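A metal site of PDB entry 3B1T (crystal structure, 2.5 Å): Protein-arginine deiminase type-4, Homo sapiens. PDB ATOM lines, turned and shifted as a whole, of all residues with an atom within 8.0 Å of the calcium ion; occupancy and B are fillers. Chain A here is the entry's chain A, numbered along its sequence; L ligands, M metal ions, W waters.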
ATOM      1  N   MET A 306     -25.655 -27.901  -1.150  1.00  0.00           N
ATOM      2  CA  MET A 306     -24.825 -26.729  -1.513  1.00  0.00           C
ATOM      3  C   MET A 306     -24.775 -25.730  -0.381  1.00  0.00           C
ATOM      4  O   MET A 306     -25.601 -25.755   0.523  1.00  0.00           O
ATOM      5  CB  MET A 306     -25.365 -26.024  -2.760  1.00  0.00           C
ATOM      6  CG  MET A 306     -25.210 -26.806  -4.045  1.00  0.00           C
ATOM      7  SD  MET A 306     -25.827 -26.011  -5.535  1.00  0.00           S
ATOM      8  CE  MET A 306     -24.769 -24.569  -5.628  1.00  0.00           C
ATOM      9  N   THR A 307     -23.823 -24.823  -0.448  1.00  0.00           N
ATOM     10  CA  THR A 307     -23.656 -23.790   0.563  1.00  0.00           C
ATOM     11  C   THR A 307     -23.714 -22.413  -0.090  1.00  0.00           C
ATOM     12  O   THR A 307     -22.922 -22.132  -1.001  1.00  0.00           O
ATOM     13  CB  THR A 307     -22.313 -23.932   1.264  1.00  0.00           C
ATOM     14  OG1 THR A 307     -21.279 -23.907   0.266  1.00  0.00           O
ATOM     15  CG2 THR A 307     -22.261 -25.245   2.051  1.00  0.00           C
ATOM     16  N   ASN A 309     -23.610 -18.128  -0.520  1.00  0.00           N
ATOM     17  CA  ASN A 309     -22.574 -17.124  -0.251  1.00  0.00           C
ATOM     18  C   ASN A 309     -22.642 -16.573   1.170  1.00  0.00           C
ATOM     19  O   ASN A 309     -21.732 -15.885   1.617  1.00  0.00           O
ATOM     20  CB  ASN A 309     -22.704 -15.958  -1.213  1.00  0.00           C
ATOM     21  CG  ASN A 309     -22.475 -16.369  -2.647  1.00  0.00           C
ATOM     22  OD1 ASN A 309     -22.015 -17.470  -2.920  1.00  0.00           O
ATOM     23  ND2 ASN A 309     -22.785 -15.459  -3.579  1.00  0.00           N
ATOM     24  N   MET A 356     -13.121 -21.201 -13.523  1.00  0.00           N
ATOM     25  CA  MET A 356     -13.065 -22.113 -12.357  1.00  0.00           C
ATOM     26  C   MET A 356     -14.436 -22.265 -11.631  1.00  0.00           C
ATOM     27  O   MET A 356     -14.639 -23.191 -10.832  1.00  0.00           O
ATOM     28  CB  MET A 356     -11.949 -21.628 -11.406  1.00  0.00           C
ATOM     29  CG  MET A 356     -11.551 -22.598 -10.265  1.00  0.00           C
ATOM     30  SD  MET A 356     -11.086 -24.265 -10.763  1.00  0.00           S
ATOM     31  CE  MET A 356      -9.301 -24.154 -10.910  1.00  0.00           C
ATOM     32  N   GLN A 357     -15.344 -21.345 -11.927  1.00  0.00           N
ATOM     33  CA  GLN A 357     -16.717 -21.379 -11.484  1.00  0.00           C
ATOM     34  C   GLN A 357     -17.549 -22.450 -12.184  1.00  0.00           C
ATOM     35  O   GLN A 357     -18.519 -22.983 -11.622  1.00  0.00           O
ATOM     36  CB  GLN A 357     -17.349 -20.005 -11.768  1.00  0.00           C
ATOM     37  CG  GLN A 357     -18.844 -19.841 -11.481  1.00  0.00           C
ATOM     38  CD  GLN A 357     -19.250 -20.269 -10.102  1.00  0.00           C
ATOM     39  OE1 GLN A 357     -20.333 -20.822  -9.934  1.00  0.00           O
ATOM     40  NE2 GLN A 357     -18.415 -20.002  -9.101  1.00  0.00           N
ATOM     41  N   ASP A 358     -17.174 -22.752 -13.415  1.00  0.00           N
ATOM     42  CA  ASP A 358     -18.038 -23.515 -14.304  1.00  0.00           C
ATOM     43  C   ASP A 358     -17.929 -25.053 -14.204  1.00  0.00           C
ATOM     44  O   ASP A 358     -18.948 -25.723 -14.328  1.00  0.00           O
ATOM     45  CB  ASP A 358     -17.798 -23.068 -15.742  1.00  0.00           C
ATOM     46  CG  ASP A 358     -18.177 -21.612 -15.958  1.00  0.00           C
ATOM     47  OD1 ASP A 358     -18.854 -21.006 -15.100  1.00  0.00           O
ATOM     48  OD2 ASP A 358     -17.800 -21.069 -17.009  1.00  0.00           O
ATOM     49  N   MET A 360     -17.066 -27.112 -11.649  1.00  0.00           N
ATOM     50  CA  MET A 360     -17.435 -27.791 -10.419  1.00  0.00           C
ATOM     51  C   MET A 360     -18.256 -26.921  -9.463  1.00  0.00           C
ATOM     52  O   MET A 360     -18.337 -25.701  -9.607  1.00  0.00           O
ATOM     53  CB  MET A 360     -16.157 -28.261  -9.729  1.00  0.00           C
ATOM     54  CG  MET A 360     -15.374 -27.126  -9.135  1.00  0.00           C
ATOM     55  SD  MET A 360     -13.864 -27.610  -8.292  1.00  0.00           S
ATOM     56  CE  MET A 360     -13.450 -26.015  -7.591  1.00  0.00           C
ATOM     57  N   GLU A 361     -18.858 -27.589  -8.464  1.00  0.00           N
ATOM     58  CA  GLU A 361     -19.553 -26.934  -7.340  1.00  0.00           C
ATOM     59  C   GLU A 361     -19.207 -27.715  -6.082  1.00  0.00           C
ATOM     60  O   GLU A 361     -19.406 -28.903  -6.027  1.00  0.00           O
ATOM     61  CB  GLU A 361     -21.079 -26.925  -7.587  1.00  0.00           C
ATOM     62  CG  GLU A 361     -21.950 -26.152  -6.591  1.00  0.00           C
ATOM     63  CD  GLU A 361     -21.888 -24.629  -6.737  1.00  0.00           C
ATOM     64  OE1 GLU A 361     -22.030 -24.091  -7.865  1.00  0.00           O
ATOM     65  OE2 GLU A 361     -21.712 -23.963  -5.692  1.00  0.00           O
ATOM     66  N   ILE A 362     -18.647 -27.053  -5.088  1.00  0.00           N
ATOM     67  CA  ILE A 362     -18.242 -27.734  -3.865  1.00  0.00           C
ATOM     68  C   ILE A 362     -19.395 -27.713  -2.867  1.00  0.00           C
ATOM     69  O   ILE A 362     -19.831 -26.641  -2.445  1.00  0.00           O
ATOM     70  CB  ILE A 362     -17.004 -27.086  -3.174  1.00  0.00           C
ATOM     71  CG1 ILE A 362     -15.902 -26.728  -4.175  1.00  0.00           C
ATOM     72  CG2 ILE A 362     -16.463 -28.027  -2.096  1.00  0.00           C
ATOM     73  CD1 ILE A 362     -15.421 -27.876  -5.040  1.00  0.00           C
ATOM     74  N   SER A 414     -22.975 -25.486 -17.264  1.00  0.00           N
ATOM     75  CA  SER A 414     -21.860 -24.978 -16.482  1.00  0.00           C
ATOM     76  C   SER A 414     -22.370 -24.445 -15.131  1.00  0.00           C
ATOM     77  O   SER A 414     -23.511 -23.991 -15.012  1.00  0.00           O
ATOM     78  CB  SER A 414     -21.152 -23.864 -17.253  1.00  0.00           C
ATOM     79  OG  SER A 414     -20.548 -24.350 -18.458  1.00  0.00           O
ATOM     80  N   PHE A 415     -21.519 -24.513 -14.123  1.00  0.00           N
ATOM     81  CA  PHE A 415     -21.951 -24.349 -12.730  1.00  0.00           C
ATOM     82  C   PHE A 415     -21.911 -22.931 -12.235  1.00  0.00           C
ATOM     83  O   PHE A 415     -22.147 -22.669 -11.059  1.00  0.00           O
ATOM     84  CB  PHE A 415     -21.164 -25.308 -11.841  1.00  0.00           C
ATOM     85  CG  PHE A 415     -21.631 -26.752 -11.946  1.00  0.00           C
ATOM     86  CD1 PHE A 415     -21.281 -27.670 -10.984  1.00  0.00           C
ATOM     87  CD2 PHE A 415     -22.466 -27.170 -12.989  1.00  0.00           C
ATOM     88  CE1 PHE A 415     -21.728 -28.975 -11.053  1.00  0.00           C
ATOM     89  CE2 PHE A 415     -22.928 -28.468 -13.059  1.00  0.00           C
ATOM     90  CZ  PHE A 415     -22.549 -29.376 -12.094  1.00  0.00           C
ATOM     91  N   GLY A 416     -21.668 -21.995 -13.142  1.00  0.00           N
ATOM     92  CA  GLY A 416     -22.084 -20.610 -12.955  1.00  0.00           C
ATOM     93  C   GLY A 416     -23.588 -20.488 -13.022  1.00  0.00           C
ATOM     94  O   GLY A 416     -24.155 -19.482 -12.577  1.00  0.00           O
ATOM     95  N   ASN A 417     -24.212 -21.512 -13.616  1.00  0.00           N
ATOM     96  CA  ASN A 417     -25.657 -21.634 -13.664  1.00  0.00           C
ATOM     97  C   ASN A 417     -26.206 -22.509 -12.536  1.00  0.00           C
ATOM     98  O   ASN A 417     -27.332 -23.004 -12.651  1.00  0.00           O
ATOM     99  CB  ASN A 417     -26.124 -22.244 -15.000  1.00  0.00           C
ATOM    100  CG  ASN A 417     -27.529 -21.806 -15.380  1.00  0.00           C
ATOM    101  OD1 ASN A 417     -27.943 -20.713 -15.007  1.00  0.00           O
ATOM    102  ND2 ASN A 417     -28.261 -22.649 -16.087  1.00  0.00           N
ATOM    103  N   LEU A 418     -25.439 -22.711 -11.479  1.00  0.00           N
ATOM    104  CA  LEU A 418     -25.953 -23.361 -10.283  1.00  0.00           C
ATOM    105  C   LEU A 418     -25.641 -22.538  -9.015  1.00  0.00           C
ATOM    106  O   LEU A 418     -24.483 -22.380  -8.644  1.00  0.00           O
ATOM    107  CB  LEU A 418     -25.321 -24.713 -10.168  1.00  0.00           C
ATOM    108  CG  LEU A 418     -25.989 -25.742  -9.282  1.00  0.00           C
ATOM    109  CD1 LEU A 418     -27.355 -26.101  -9.825  1.00  0.00           C
ATOM    110  CD2 LEU A 418     -25.111 -26.917  -9.285  1.00  0.00           C
ATOM    111  N   GLU A 419     -26.682 -22.012  -8.365  1.00  0.00           N
ATOM    112  CA  GLU A 419     -26.510 -21.300  -7.084  1.00  0.00           C
ATOM    113  C   GLU A 419     -27.435 -21.886  -5.992  1.00  0.00           C
ATOM    114  O   GLU A 419     -28.196 -22.791  -6.267  1.00  0.00           O
ATOM    115  CB  GLU A 419     -26.783 -19.828  -7.315  1.00  0.00           C
ATOM    116  CG  GLU A 419     -25.827 -19.189  -8.373  1.00  0.00           C
ATOM    117  CD  GLU A 419     -24.404 -19.073  -7.865  1.00  0.00           C
ATOM    118  OE1 GLU A 419     -23.461 -19.590  -8.521  1.00  0.00           O
ATOM    119  OE2 GLU A 419     -24.252 -18.458  -6.759  1.00  0.00           O
ATOM    120  N   VAL A 420     -27.272 -21.448  -4.750  1.00  0.00           N
ATOM    121  CA  VAL A 420     -28.284 -21.664  -3.681  1.00  0.00           C
ATOM    122  C   VAL A 420     -28.571 -20.352  -3.081  1.00  0.00           C
ATOM    123  O   VAL A 420     -27.641 -19.556  -2.845  1.00  0.00           O
ATOM    124  CB  VAL A 420     -27.807 -22.413  -2.402  1.00  0.00           C
ATOM    125  CG1 VAL A 420     -28.518 -23.672  -2.215  1.00  0.00           C
ATOM    126  CG2 VAL A 420     -26.332 -22.568  -2.339  1.00  0.00           C
ATOM    127  N   LEU A 437     -31.037 -22.731  -7.085  1.00  0.00           N
ATOM    128  CA  LEU A 437     -31.445 -21.876  -8.173  1.00  0.00           C
ATOM    129  C   LEU A 437     -30.679 -22.267  -9.421  1.00  0.00           C
ATOM    130  O   LEU A 437     -29.449 -22.336  -9.398  1.00  0.00           O
ATOM    131  CB  LEU A 437     -30.992 -20.463  -7.853  1.00  0.00           C
ATOM    132  CG  LEU A 437     -31.766 -19.461  -6.971  1.00  0.00           C
ATOM    133  CD1 LEU A 437     -32.900 -20.075  -6.178  1.00  0.00           C
ATOM    134  CD2 LEU A 437     -30.747 -18.695  -6.135  1.00  0.00           C
ATOM    135  N   HIS A 479     -25.962 -17.842 -17.573  1.00  0.00           N
ATOM    136  CA  HIS A 479     -25.795 -18.230 -16.176  1.00  0.00           C
ATOM    137  C   HIS A 479     -26.460 -17.270 -15.212  1.00  0.00           C
ATOM    138  O   HIS A 479     -26.277 -16.045 -15.335  1.00  0.00           O
ATOM    139  CB  HIS A 479     -24.323 -18.250 -15.816  1.00  0.00           C
ATOM    140  CG  HIS A 479     -23.522 -19.253 -16.561  1.00  0.00           C
ATOM    141  ND1 HIS A 479     -22.228 -19.568 -16.213  1.00  0.00           N
ATOM    142  CD2 HIS A 479     -23.821 -20.028 -17.635  1.00  0.00           C
ATOM    143  CE1 HIS A 479     -21.756 -20.467 -17.052  1.00  0.00           C
ATOM    144  NE2 HIS A 479     -22.705 -20.760 -17.921  1.00  0.00           N
ATOM    145  N   VAL A 480     -27.140 -17.818 -14.208  1.00  0.00           N
ATOM    146  CA  VAL A 480     -27.746 -16.995 -13.160  1.00  0.00           C
ATOM    147  C   VAL A 480     -26.773 -16.075 -12.406  1.00  0.00           C
ATOM    148  O   VAL A 480     -27.229 -15.042 -11.887  1.00  0.00           O
ATOM    149  CB  VAL A 480     -28.583 -17.814 -12.101  1.00  0.00           C
ATOM    150  CG1 VAL A 480     -29.904 -18.367 -12.713  1.00  0.00           C
ATOM    151  CG2 VAL A 480     -27.773 -18.896 -11.515  1.00  0.00           C
ATOM    152  N   ASP A 481     -25.465 -16.408 -12.329  1.00  0.00           N
ATOM    153  CA  ASP A 481     -24.502 -15.529 -11.614  1.00  0.00           C
ATOM    154  C   ASP A 481     -24.234 -14.274 -12.403  1.00  0.00           C
ATOM    155  O   ASP A 481     -23.688 -13.317 -11.881  1.00  0.00           O
ATOM    156  CB  ASP A 481     -23.197 -16.229 -11.131  1.00  0.00           C
ATOM    157  CG  ASP A 481     -22.300 -16.767 -12.280  1.00  0.00           C
ATOM    158  OD1 ASP A 481     -21.120 -17.155 -12.000  1.00  0.00           O
ATOM    159  OD2 ASP A 481     -22.737 -16.807 -13.451  1.00  0.00           O
ATOM    160  N   HIS A 652     -16.361 -13.653 -10.429  1.00  0.00           N
ATOM    161  CA  HIS A 652     -17.100 -14.827  -9.937  1.00  0.00           C
ATOM    162  C   HIS A 652     -16.903 -16.003 -10.891  1.00  0.00           C
ATOM    163  O   HIS A 652     -16.754 -17.139 -10.441  1.00  0.00           O
ATOM    164  CB  HIS A 652     -18.588 -14.536  -9.737  1.00  0.00           C
ATOM    165  CG  HIS A 652     -19.314 -15.634  -9.026  1.00  0.00           C
ATOM    166  ND1 HIS A 652     -20.096 -16.556  -9.687  1.00  0.00           N
ATOM    167  CD2 HIS A 652     -19.374 -15.960  -7.710  1.00  0.00           C
ATOM    168  CE1 HIS A 652     -20.611 -17.408  -8.811  1.00  0.00           C
ATOM    169  NE2 HIS A 652     -20.195 -17.063  -7.598  1.00  0.00           N
ATOM    170  N   THR A 655     -13.416 -18.070 -10.669  1.00  0.00           N
ATOM    171  CA  THR A 655     -13.126 -18.580  -9.296  1.00  0.00           C
ATOM    172  C   THR A 655     -14.173 -19.508  -8.693  1.00  0.00           C
ATOM    173  O   THR A 655     -15.294 -19.598  -9.178  1.00  0.00           O
ATOM    174  CB  THR A 655     -12.984 -17.410  -8.253  1.00  0.00           C
ATOM    175  OG1 THR A 655     -14.230 -16.697  -8.151  1.00  0.00           O
ATOM    176  CG2 THR A 655     -11.874 -16.433  -8.641  1.00  0.00           C
ATOM    177  N   ASN A 656     -13.786 -20.184  -7.604  1.00  0.00           N
ATOM    178  CA  ASN A 656     -14.709 -20.980  -6.773  1.00  0.00           C
ATOM    179  C   ASN A 656     -14.375 -20.910  -5.281  1.00  0.00           C
ATOM    180  O   ASN A 656     -13.300 -20.461  -4.903  1.00  0.00           O
ATOM    181  CB  ASN A 656     -14.756 -22.447  -7.247  1.00  0.00           C
ATOM    182  CG  ASN A 656     -16.178 -22.934  -7.411  1.00  0.00           C
ATOM    183  OD1 ASN A 656     -17.049 -22.563  -6.632  1.00  0.00           O
ATOM    184  ND2 ASN A 656     -16.426 -23.729  -8.440  1.00  0.00           N
ATOM    185  N   ARG A 659     -17.267 -23.591   1.354  1.00  0.00           N
ATOM    186  CA  ARG A 659     -17.764 -22.893   2.526  1.00  0.00           C
ATOM    187  C   ARG A 659     -18.255 -23.827   3.617  1.00  0.00           C
ATOM    188  O   ARG A 659     -18.470 -25.017   3.399  1.00  0.00           O
ATOM    189  CB  ARG A 659     -18.911 -21.963   2.127  1.00  0.00           C
ATOM    190  CG  ARG A 659     -18.626 -21.112   0.911  1.00  0.00           C
ATOM    191  CD  ARG A 659     -19.764 -20.187   0.613  1.00  0.00           C
ATOM    192  NE  ARG A 659     -19.274 -18.911   0.070  1.00  0.00           N
ATOM    193  CZ  ARG A 659     -19.242 -18.599  -1.219  1.00  0.00           C
ATOM    194  NH1 ARG A 659     -19.689 -19.450  -2.133  1.00  0.00           N
ATOM    195  NH2 ARG A 659     -18.774 -17.431  -1.603  1.00  0.00           N
HETATM  196  C1  LIG L   1     -12.516 -19.327 -23.873  1.00  0.00           C
HETATM  197  O1  LIG L   1     -12.587 -20.480 -24.364  1.00  0.00           O
HETATM  198  O2  LIG L   1     -11.817 -19.085 -22.861  1.00  0.00           O
HETATM  199  N1  LIG L   1     -18.781 -18.614 -22.716  1.00  0.00           N
HETATM  200  N2  LIG L   1     -19.897 -18.514 -15.307  1.00  0.00           N
HETATM  201  O3  LIG L   1     -18.870 -20.327 -21.300  1.00  0.00           O
HETATM  202  O4  LIG L   1     -15.500 -20.019 -23.505  1.00  0.00           O
HETATM  203  C2  LIG L   1     -13.283 -16.384 -26.150  1.00  0.00           C
HETATM  204  C3  LIG L   1     -12.612 -17.422 -25.486  1.00  0.00           C
HETATM  205  C4  LIG L   1     -14.629 -16.146 -25.879  1.00  0.00           C
HETATM  206  C5  LIG L   1     -13.280 -18.218 -24.545  1.00  0.00           C
HETATM  207  C6  LIG L   1     -15.298 -16.934 -24.944  1.00  0.00           C
HETATM  208  C7  LIG L   1     -18.266 -17.753 -19.348  1.00  0.00           C
HETATM  209  C8  LIG L   1     -18.322 -18.328 -17.930  1.00  0.00           C
HETATM  210  C9  LIG L   1     -16.934 -18.003 -20.056  1.00  0.00           C
HETATM  211  C10 LIG L   1     -20.086 -16.106 -15.322  1.00  0.00           C
HETATM  212  N3  LIG L   1     -18.906 -17.299 -17.076  1.00  0.00           N
HETATM  213  N4  LIG L   1     -16.066 -18.233 -22.259  1.00  0.00           N
HETATM  214  C11 LIG L   1     -18.252 -19.366 -21.754  1.00  0.00           C
HETATM  215  C12 LIG L   1     -19.615 -17.387 -15.943  1.00  0.00           C
HETATM  216  C13 LIG L   1     -15.428 -18.806 -23.292  1.00  0.00           C
HETATM  217  C14 LIG L   1     -14.633 -17.968 -24.271  1.00  0.00           C
HETATM  218  C15 LIG L   1     -16.882 -18.953 -21.261  1.00  0.00           C
HETATM  219 CA    CA M   1     -22.065 -21.905  -8.856  1.00  0.00          CA
HETATM  220  O   HOH W   1     -19.876 -23.113  -8.957  1.00  0.00           O
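The side-chain carboxylate (OD1) of Asp 481 lies within salt-bridge range of a nitrogen (N2) of the ligand (3.8 Å). N2 of the ligand is in salt-bridge range of OD1 of Asp 358 (2.7 Å). ND1 of His 479 is in hydrogen-bond range of N2 of the ligand, at 2.7 Å.
Of the 24 residues printed, 5 come within 4 Å of the calcium ion. The nearest printed residue that does not touch the calcium ion is Gly 416 (4.3 Å).
The calcium ion is bound by OE1 of Gln 357, O of Phe 415, OE1 of Glu 361, O of Leu 418, water W1 and OE1 of Glu 419.
The backbone NH (N) of Phe 415 sits at hydrogen-bond distance from the backbone carbonyl oxygen (O) of Asp 358, at 2.8 Å. The side-chain amide nitrogen (NE2) of Gln 357 sits at hydrogen-bond distance from the backbone carbonyl oxygen (O) of Thr 655 (3.1 Å). O of Glu 419 is in hydrogen-bond range of N of Leu 437, at 3.0 Å.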
